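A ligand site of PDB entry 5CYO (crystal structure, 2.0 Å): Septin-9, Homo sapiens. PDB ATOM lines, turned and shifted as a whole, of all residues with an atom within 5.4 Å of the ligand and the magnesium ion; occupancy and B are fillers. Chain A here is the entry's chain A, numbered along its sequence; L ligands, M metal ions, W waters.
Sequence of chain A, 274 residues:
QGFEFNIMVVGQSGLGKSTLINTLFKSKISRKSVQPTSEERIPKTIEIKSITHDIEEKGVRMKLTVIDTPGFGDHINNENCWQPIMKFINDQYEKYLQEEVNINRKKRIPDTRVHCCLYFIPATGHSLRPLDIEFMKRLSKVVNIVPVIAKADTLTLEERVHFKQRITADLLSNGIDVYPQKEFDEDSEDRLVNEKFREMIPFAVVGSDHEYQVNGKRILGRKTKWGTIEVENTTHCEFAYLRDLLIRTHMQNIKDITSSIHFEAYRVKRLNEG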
ATOM      1  N   GLN A  12      12.878  10.400 -23.781  1.00  0.00           N
ATOM      2  CA  GLN A  12      13.692  10.454 -22.594  1.00  0.00           C
ATOM      3  C   GLN A  12      15.067  11.035 -22.916  1.00  0.00           C
ATOM      4  O   GLN A  12      15.499  10.930 -24.018  1.00  0.00           O
ATOM      5  CB  GLN A  12      13.897   9.053 -22.039  1.00  0.00           C
ATOM      6  CG  GLN A  12      12.679   8.302 -21.589  1.00  0.00           C
ATOM      7  CD  GLN A  12      13.007   6.998 -20.883  1.00  0.00           C
ATOM      8  OE1 GLN A  12      12.159   6.362 -20.377  1.00  0.00           O
ATOM      9  NE2 GLN A  12      14.247   6.588 -20.907  1.00  0.00           N
ATOM     10  N   SER A  13      15.732  11.639 -21.928  1.00  0.00           N
ATOM     11  CA  SER A  13      17.069  12.176 -22.075  1.00  0.00           C
ATOM     12  C   SER A  13      18.065  11.066 -22.390  1.00  0.00           C
ATOM     13  O   SER A  13      17.838   9.901 -22.053  1.00  0.00           O
ATOM     14  CB  SER A  13      17.508  12.908 -20.810  1.00  0.00           C
ATOM     15  OG  SER A  13      16.634  13.982 -20.531  1.00  0.00           O
ATOM     16  N   GLY A  14      19.162  11.446 -23.029  1.00  0.00           N
ATOM     17  CA  GLY A  14      20.228  10.500 -23.305  1.00  0.00           C
ATOM     18  C   GLY A  14      19.904   9.542 -24.432  1.00  0.00           C
ATOM     19  O   GLY A  14      20.473   8.456 -24.505  1.00  0.00           O
ATOM     20  N   LEU A  15      18.975   9.933 -25.308  1.00  0.00           N
ATOM     21  CA  LEU A  15      18.632   9.081 -26.436  1.00  0.00           C
ATOM     22  C   LEU A  15      19.201   9.625 -27.752  1.00  0.00           C
ATOM     23  O   LEU A  15      18.939   9.085 -28.827  1.00  0.00           O
ATOM     24  CB  LEU A  15      17.112   8.924 -26.554  1.00  0.00           C
ATOM     25  CG  LEU A  15      16.436   8.131 -25.429  1.00  0.00           C
ATOM     26  CD1 LEU A  15      14.957   7.930 -25.720  1.00  0.00           C
ATOM     27  CD2 LEU A  15      17.141   6.802 -25.182  1.00  0.00           C
ATOM     28  N   GLY A  16      19.999  10.691 -27.657  1.00  0.00           N
ATOM     29  CA  GLY A  16      20.622  11.268 -28.843  1.00  0.00           C
ATOM     30  C   GLY A  16      19.716  12.234 -29.587  1.00  0.00           C
ATOM     31  O   GLY A  16      19.932  12.492 -30.785  1.00  0.00           O
ATOM     32  N   LYS A  17      18.712  12.777 -28.906  1.00  0.00           N
ATOM     33  CA  LYS A  17      17.756  13.681 -29.536  1.00  0.00           C
ATOM     34  C   LYS A  17      18.407  14.978 -29.998  1.00  0.00           C
ATOM     35  O   LYS A  17      18.229  15.391 -31.143  1.00  0.00           O
ATOM     36  CB  LYS A  17      16.612  14.015 -28.575  1.00  0.00           C
ATOM     37  CG  LYS A  17      15.773  12.818 -28.144  1.00  0.00           C
ATOM     38  CD  LYS A  17      14.515  13.287 -27.406  1.00  0.00           C
ATOM     39  CE  LYS A  17      14.867  14.116 -26.174  1.00  0.00           C
ATOM     40  NZ  LYS A  17      15.813  13.379 -25.251  1.00  0.00           N
ATOM     41  N   SER A  18      19.150  15.633 -29.119  1.00  0.00           N
ATOM     42  CA  SER A  18      19.777  16.899 -29.469  1.00  0.00           C
ATOM     43  C   SER A  18      20.828  16.682 -30.546  1.00  0.00           C
ATOM     44  O   SER A  18      21.019  17.518 -31.429  1.00  0.00           O
ATOM     45  CB  SER A  18      20.394  17.558 -28.228  1.00  0.00           C
ATOM     46  OG  SER A  18      19.398  17.871 -27.281  1.00  0.00           O
ATOM     47  N   THR A  19      21.505  15.533 -30.480  1.00  0.00           N
ATOM     48  CA  THR A  19      22.480  15.159 -31.493  1.00  0.00           C
ATOM     49  C   THR A  19      21.844  14.996 -32.872  1.00  0.00           C
ATOM     50  O   THR A  19      22.369  15.481 -33.878  1.00  0.00           O
ATOM     51  CB  THR A  19      23.191  13.833 -31.124  1.00  0.00           C
ATOM     52  OG1 THR A  19      23.866  13.965 -29.862  1.00  0.00           O
ATOM     53  CG2 THR A  19      24.193  13.439 -32.210  1.00  0.00           C
ATOM     54  N   LEU A  20      20.701  14.323 -32.922  1.00  0.00           N
ATOM     55  CA  LEU A  20      20.028  14.058 -34.189  1.00  0.00           C
ATOM     56  C   LEU A  20      19.511  15.350 -34.832  1.00  0.00           C
ATOM     57  O   LEU A  20      19.434  15.450 -36.054  1.00  0.00           O
ATOM     58  CB  LEU A  20      18.888  13.065 -34.021  1.00  0.00           C
ATOM     59  CG  LEU A  20      18.525  12.393 -35.353  1.00  0.00           C
ATOM     60  CD1 LEU A  20      19.655  11.466 -35.797  1.00  0.00           C
ATOM     61  CD2 LEU A  20      17.205  11.639 -35.279  1.00  0.00           C
ATOM     62  N   ILE A  42      27.180  18.261 -26.391  1.00  0.00           N
ATOM     63  CA  ILE A  42      25.909  18.940 -26.163  1.00  0.00           C
ATOM     64  C   ILE A  42      25.431  18.803 -24.717  1.00  0.00           C
ATOM     65  O   ILE A  42      25.340  17.688 -24.201  1.00  0.00           O
ATOM     66  CB  ILE A  42      24.819  18.387 -27.096  1.00  0.00           C
ATOM     67  CG1 ILE A  42      25.269  18.490 -28.552  1.00  0.00           C
ATOM     68  CG2 ILE A  42      23.504  19.103 -26.867  1.00  0.00           C
ATOM     69  CD1 ILE A  42      24.308  17.839 -29.526  1.00  0.00           C
ATOM     70  N   PRO A  43      25.118  19.926 -24.075  1.00  0.00           N
ATOM     71  CA  PRO A  43      24.602  19.853 -22.708  1.00  0.00           C
ATOM     72  C   PRO A  43      23.256  19.141 -22.666  1.00  0.00           C
ATOM     73  O   PRO A  43      22.557  19.082 -23.674  1.00  0.00           O
ATOM     74  CB  PRO A  43      24.444  21.330 -22.309  1.00  0.00           C
ATOM     75  CG  PRO A  43      25.288  22.091 -23.273  1.00  0.00           C
ATOM     76  CD  PRO A  43      25.240  21.310 -24.544  1.00  0.00           C
ATOM     77  N   LYS A  44      22.902  18.585 -21.501  1.00  0.00           N
ATOM     78  CA  LYS A  44      21.575  18.024 -21.322  1.00  0.00           C
ATOM     79  C   LYS A  44      20.535  19.110 -21.541  1.00  0.00           C
ATOM     80  O   LYS A  44      20.684  20.222 -21.047  1.00  0.00           O
ATOM     81  CB  LYS A  44      21.408  17.426 -19.918  1.00  0.00           C
ATOM     82  CG  LYS A  44      20.056  16.757 -19.751  1.00  0.00           C
ATOM     83  CD  LYS A  44      19.546  16.878 -18.326  1.00  0.00           C
ATOM     84  CE  LYS A  44      19.638  15.564 -17.593  1.00  0.00           C
ATOM     85  NZ  LYS A  44      19.121  15.667 -16.192  1.00  0.00           N
ATOM     86  N   THR A  45      19.486  18.782 -22.275  1.00  0.00           N
ATOM     87  CA  THR A  45      18.438  19.750 -22.610  1.00  0.00           C
ATOM     88  C   THR A  45      17.455  19.898 -21.459  1.00  0.00           C
ATOM     89  O   THR A  45      16.748  18.950 -21.125  1.00  0.00           O
ATOM     90  CB  THR A  45      17.671  19.320 -23.867  1.00  0.00           C
ATOM     91  OG1 THR A  45      18.602  18.887 -24.884  1.00  0.00           O
ATOM     92  CG2 THR A  45      16.818  20.461 -24.398  1.00  0.00           C
ATOM     93  N   ASP A  68      13.689  21.291 -29.669  1.00  0.00           N
ATOM     94  CA  ASP A  68      14.349  20.398 -28.721  1.00  0.00           C
ATOM     95  C   ASP A  68      13.580  20.433 -27.404  1.00  0.00           C
ATOM     96  O   ASP A  68      13.076  21.485 -27.016  1.00  0.00           O
ATOM     97  CB  ASP A  68      15.806  20.792 -28.506  1.00  0.00           C
ATOM     98  CG  ASP A  68      16.682  19.603 -28.116  1.00  0.00           C
ATOM     99  OD1 ASP A  68      16.126  18.522 -27.833  1.00  0.00           O
ATOM    100  OD2 ASP A  68      17.924  19.756 -28.075  1.00  0.00           O
ATOM    101  N   THR A  69      13.541  19.304 -26.705  1.00  0.00           N
ATOM    102  CA  THR A  69      12.735  19.175 -25.497  1.00  0.00           C
ATOM    103  C   THR A  69      13.495  18.535 -24.343  1.00  0.00           C
ATOM    104  O   THR A  69      14.402  17.744 -24.577  1.00  0.00           O
ATOM    105  CB  THR A  69      11.470  18.336 -25.744  1.00  0.00           C
ATOM    106  OG1 THR A  69      11.847  17.056 -26.274  1.00  0.00           O
ATOM    107  CG2 THR A  69      10.532  19.040 -26.713  1.00  0.00           C
ATOM    108  N   LYS A 151      19.617   5.719 -31.017  1.00  0.00           N
ATOM    109  CA  LYS A 151      20.922   5.056 -30.933  1.00  0.00           C
ATOM    110  C   LYS A 151      20.885   3.643 -31.507  1.00  0.00           C
ATOM    111  O   LYS A 151      21.300   2.700 -30.860  1.00  0.00           O
ATOM    112  CB  LYS A 151      21.416   4.995 -29.489  1.00  0.00           C
ATOM    113  CG  LYS A 151      21.556   6.346 -28.812  1.00  0.00           C
ATOM    114  CD  LYS A 151      22.134   6.165 -27.411  1.00  0.00           C
ATOM    115  CE  LYS A 151      22.391   7.481 -26.732  1.00  0.00           C
ATOM    116  NZ  LYS A 151      23.007   7.274 -25.385  1.00  0.00           N
ATOM    117  N   ALA A 152      20.384   3.532 -32.729  1.00  0.00           N
ATOM    118  CA  ALA A 152      20.100   2.242 -33.343  1.00  0.00           C
ATOM    119  C   ALA A 152      21.349   1.395 -33.552  1.00  0.00           C
ATOM    120  O   ALA A 152      21.265   0.182 -33.776  1.00  0.00           O
ATOM    121  CB  ALA A 152      19.381   2.436 -34.664  1.00  0.00           C
ATOM    122  N   ASP A 153      22.512   2.030 -33.454  1.00  0.00           N
ATOM    123  CA  ASP A 153      23.774   1.317 -33.536  1.00  0.00           C
ATOM    124  C   ASP A 153      23.923   0.344 -32.357  1.00  0.00           C
ATOM    125  O   ASP A 153      24.778  -0.539 -32.377  1.00  0.00           O
ATOM    126  CB  ASP A 153      24.940   2.310 -33.584  1.00  0.00           C
ATOM    127  CG  ASP A 153      24.895   3.326 -32.458  1.00  0.00           C
ATOM    128  OD1 ASP A 153      23.924   4.110 -32.386  1.00  0.00           O
ATOM    129  OD2 ASP A 153      25.849   3.348 -31.653  1.00  0.00           O
ATOM    130  N   THR A 154      23.067   0.504 -31.354  1.00  0.00           N
ATOM    131  CA  THR A 154      23.034  -0.389 -30.196  1.00  0.00           C
ATOM    132  C   THR A 154      22.573  -1.788 -30.571  1.00  0.00           C
ATOM    133  O   THR A 154      22.908  -2.773 -29.916  1.00  0.00           O
ATOM    134  CB  THR A 154      22.054   0.162 -29.112  1.00  0.00           C
ATOM    135  OG1 THR A 154      22.405   1.495 -28.757  1.00  0.00           O
ATOM    136  CG2 THR A 154      22.024  -0.714 -27.869  1.00  0.00           C
ATOM    137  N   VAL A 205      17.673   5.112 -36.291  1.00  0.00           N
ATOM    138  CA  VAL A 205      18.559   6.233 -36.556  1.00  0.00           C
ATOM    139  C   VAL A 205      19.820   6.258 -35.686  1.00  0.00           C
ATOM    140  O   VAL A 205      19.852   5.715 -34.581  1.00  0.00           O
ATOM    141  CB  VAL A 205      17.850   7.583 -36.391  1.00  0.00           C
ATOM    142  CG1 VAL A 205      16.616   7.652 -37.282  1.00  0.00           C
ATOM    143  CG2 VAL A 205      17.507   7.843 -34.931  1.00  0.00           C
ATOM    144  N   VAL A 206      20.850   6.870 -36.255  1.00  0.00           N
ATOM    145  CA  VAL A 206      22.112   7.120 -35.572  1.00  0.00           C
ATOM    146  C   VAL A 206      22.486   8.593 -35.749  1.00  0.00           C
ATOM    147  O   VAL A 206      22.398   9.115 -36.856  1.00  0.00           O
ATOM    148  CB  VAL A 206      23.232   6.225 -36.150  1.00  0.00           C
ATOM    149  CG1 VAL A 206      24.557   6.518 -35.450  1.00  0.00           C
ATOM    150  CG2 VAL A 206      22.863   4.750 -36.010  1.00  0.00           C
ATOM    151  N   GLY A 207      22.885   9.249 -34.668  1.00  0.00           N
ATOM    152  CA  GLY A 207      23.277  10.652 -34.748  1.00  0.00           C
ATOM    153  C   GLY A 207      24.778  10.767 -34.948  1.00  0.00           C
ATOM    154  O   GLY A 207      25.543   9.961 -34.434  1.00  0.00           O
ATOM    155  N   ASP A 209      28.648  12.425 -34.732  1.00  0.00           N
ATOM    156  CA  ASP A 209      29.500  13.202 -33.844  1.00  0.00           C
ATOM    157  C   ASP A 209      30.709  13.790 -34.583  1.00  0.00           C
ATOM    158  O   ASP A 209      31.540  14.444 -33.982  1.00  0.00           O
ATOM    159  CB  ASP A 209      30.000  12.375 -32.648  1.00  0.00           C
ATOM    160  CG  ASP A 209      30.677  11.074 -33.057  1.00  0.00           C
ATOM    161  OD1 ASP A 209      31.010  10.895 -34.246  1.00  0.00           O
ATOM    162  OD2 ASP A 209      30.893  10.217 -32.173  1.00  0.00           O
ATOM    163  N   ARG A 222      29.338   8.664 -37.151  1.00  0.00           N
ATOM    164  CA  ARG A 222      29.556   8.426 -35.732  1.00  0.00           C
ATOM    165  C   ARG A 222      30.710   7.456 -35.530  1.00  0.00           C
ATOM    166  O   ARG A 222      30.728   6.378 -36.132  1.00  0.00           O
ATOM    167  CB  ARG A 222      28.301   7.895 -35.039  1.00  0.00           C
ATOM    168  CG  ARG A 222      28.617   7.468 -33.601  1.00  0.00           C
ATOM    169  CD  ARG A 222      27.406   7.283 -32.723  1.00  0.00           C
ATOM    170  NE  ARG A 222      27.830   6.690 -31.456  1.00  0.00           N
ATOM    171  CZ  ARG A 222      28.213   7.375 -30.391  1.00  0.00           C
ATOM    172  NH1 ARG A 222      28.206   8.707 -30.414  1.00  0.00           N
ATOM    173  NH2 ARG A 222      28.604   6.731 -29.291  1.00  0.00           N
HETATM  174  P1  LIG L   1      19.511  13.694 -25.565  1.00  0.00           P
HETATM  175  O1  LIG L   1      19.568  13.875 -24.070  1.00  0.00           O
HETATM  176  O2  LIG L   1      19.327  15.033 -26.258  1.00  0.00           O
HETATM  177  O3  LIG L   1      18.327  12.829 -25.937  1.00  0.00           O
HETATM  178  O4  LIG L   1      20.839  12.983 -26.102  1.00  0.00           O
HETATM  179  P2  LIG L   1      22.154  13.799 -26.544  1.00  0.00           P
HETATM  180  O5  LIG L   1      22.515  14.876 -25.555  1.00  0.00           O
HETATM  181  O6  LIG L   1      21.979  14.328 -27.936  1.00  0.00           O
HETATM  182  O7  LIG L   1      23.271  12.642 -26.565  1.00  0.00           O
HETATM  183  C1  LIG L   1      23.570  11.893 -25.379  1.00  0.00           C
HETATM  184  C2  LIG L   1      24.805  11.048 -25.622  1.00  0.00           C
HETATM  185  O8  LIG L   1      24.504  10.075 -26.626  1.00  0.00           O
HETATM  186  C3  LIG L   1      25.949  11.896 -26.164  1.00  0.00           C
HETATM  187  O9  LIG L   1      27.156  11.473 -25.547  1.00  0.00           O
HETATM  188  C4  LIG L   1      26.006  11.558 -27.642  1.00  0.00           C
HETATM  189  O10 LIG L   1      27.315  11.664 -28.187  1.00  0.00           O
HETATM  190  C5  LIG L   1      25.491  10.126 -27.667  1.00  0.00           C
HETATM  191  N1  LIG L   1      24.799   9.814 -28.929  1.00  0.00           N
HETATM  192  C6  LIG L   1      24.048  10.640 -29.682  1.00  0.00           C
HETATM  193  N2  LIG L   1      23.544   9.968 -30.750  1.00  0.00           N
HETATM  194  C7  LIG L   1      23.962   8.689 -30.653  1.00  0.00           C
HETATM  195  C8  LIG L   1      23.800   7.446 -31.427  1.00  0.00           C
HETATM  196  O11 LIG L   1      23.108   7.439 -32.461  1.00  0.00           O
HETATM  197  N3  LIG L   1      24.399   6.325 -30.982  1.00  0.00           N
HETATM  198  C9  LIG L   1      25.138   6.306 -29.857  1.00  0.00           C
HETATM  199  N4  LIG L   1      25.723   5.154 -29.468  1.00  0.00           N
HETATM  200  N5  LIG L   1      25.332   7.415 -29.100  1.00  0.00           N
HETATM  201  C10 LIG L   1      24.778   8.593 -29.447  1.00  0.00           C
HETATM  202 MG    MG M   1      18.995  16.884 -25.489  1.00  0.00          MG
HETATM  203  O   HOH W   1      18.661  16.228 -23.464  1.00  0.00           O
HETATM  204  O   HOH W   2      26.316   7.089 -26.481  1.00  0.00           O
HETATM  205  O   HOH W   3      16.963  16.966 -26.052  1.00  0.00           O
HETATM  206  O   HOH W   4      29.265  13.623 -26.437  1.00  0.00           O
HETATM  207  O   HOH W   5      21.121  17.013 -25.024  1.00  0.00           O
HETATM  208  O   HOH W   6      25.093  15.183 -24.979  1.00  0.00           O
HETATM  209  O   HOH W   7      21.153  10.605 -32.257  1.00  0.00           O
HETATM  210  O   HOH W   8      27.350  12.833 -30.641  1.00  0.00           O
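The magnesium ion is bound by O2 of the ligand (2.0 Å), OG of Ser 18 (2.1 Å), water W3 (2.1 Å), OG1 of Thr 45 (2.1 Å), water W1 (2.2 Å) and water W5 (2.2 Å). The magnesium ion has six donor atoms within binding distance.
N of Ser 18 is in hydrogen-bond range of O6 of the ligand (3.3 Å). The guanidinium group of Arg 222 lies close to a nitrogen (N5) of the ligand, at 3.3 Å. The side-chain amino group (NZ) of Lys 151 lies close to an oxygen (O8) of the ligand (3.4 Å). The backbone NH (N) of Thr 19 is in hydrogen-bond range of an oxygen (O6) of the ligand, at 2.9 Å. The side-chain amino group of Lys 17 is in salt-bridge range of an oxygen (O3) of the ligand (2.7 Å). The side-chain hydroxyl of Thr 19 is in hydrogen-bond range of an oxygen (O6) of the ligand (2.7 Å). An oxygen (O4) of the ligand is in hydrogen-bond range of the backbone NH (N) of Gly 16, 2.9 Å away. The backbone NH (N) of Leu 15 lies within hydrogen-bond range of an oxygen (O3) of the ligand, at 3.0 Å. OD1 of Asp 153 sits at hydrogen-bond distance from N3 of the ligand. The backbone NH (N) of Gly 14 sits at hydrogen-bond distance from an oxygen (O1) of the ligand (2.7 Å). An oxygen (O11) of the ligand lies within hydrogen-bond range of the backbone NH (N) of Gly 207 (2.9 Å). N of Lys 17 sits at hydrogen-bond distance from O3 of the ligand.
Gln 12 touches the ligand (O to O3, 3.9 Å). Ser 13 touches the ligand. CA of Val 206 touches O11 of the ligand, 3.3 Å away. Hydrophobic or aromatic side chains within 4 Å of the ligand: Val 206. Of the 24 residues printed, 13 come within 4 Å of the ligand. The nearest printed residue that does not touch the ligand is Thr 45 (4.2 Å).
Of the 24 residues printed, 2 come within 4 Å of the magnesium ion. The nearest printed residue that does not touch the magnesium ion is Asp 68 (4.01 Å).
OD2 of Asp 153 is in salt-bridge range of NE of Arg 222 (3.9 Å). OG1 of Thr 45 lies close to OD2 of Asp 68, at 3.4 Å. NZ of Lys 151 is in hydrogen-bond range of O of Gly 14, 2.9 Å away. The guanidinium group (NH1) of Arg 222 is in salt-bridge range of the side-chain carboxylate (OD2) of Asp 209, 3.5 Å away. O of Gln 12 is in hydrogen-bond range of NZ of Lys 17, at 2.8 Å. The side-chain hydroxyl of Ser 18 lies close to the side-chain carboxylate of Asp 68. The backbone carbonyl oxygen (O) of Lys 151 lies within hydrogen-bond range of the side-chain hydroxyl (OG1) of Thr 154 (2.7 Å).
Water W5 bridges O5 of the ligand (2.6 Å) and O of Pro 43 (2.9 Å). Water W3 lies within hydrogen-bond range of OD1 of Asp 68 (2.5 Å) and O of Thr 69 (3.1 Å). Water W1 bridges an oxygen (O1) of the ligand (2.6 Å) and the backbone NH (N) of Thr 45 (2.9 Å). Water W6 bridges O of Ile 42 (2.6 Å) and O5 of the ligand (2.7 Å). Water W2 lies within hydrogen-bond range of N5 of the ligand (2.8 Å) and NZ of Lys 151 (3.5 Å). Water W7 lies within hydrogen-bond range of O of Gly 16 (2.7 Å), N2 of the ligand (2.9 Å) and N of Gly 207 (3.3 Å).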
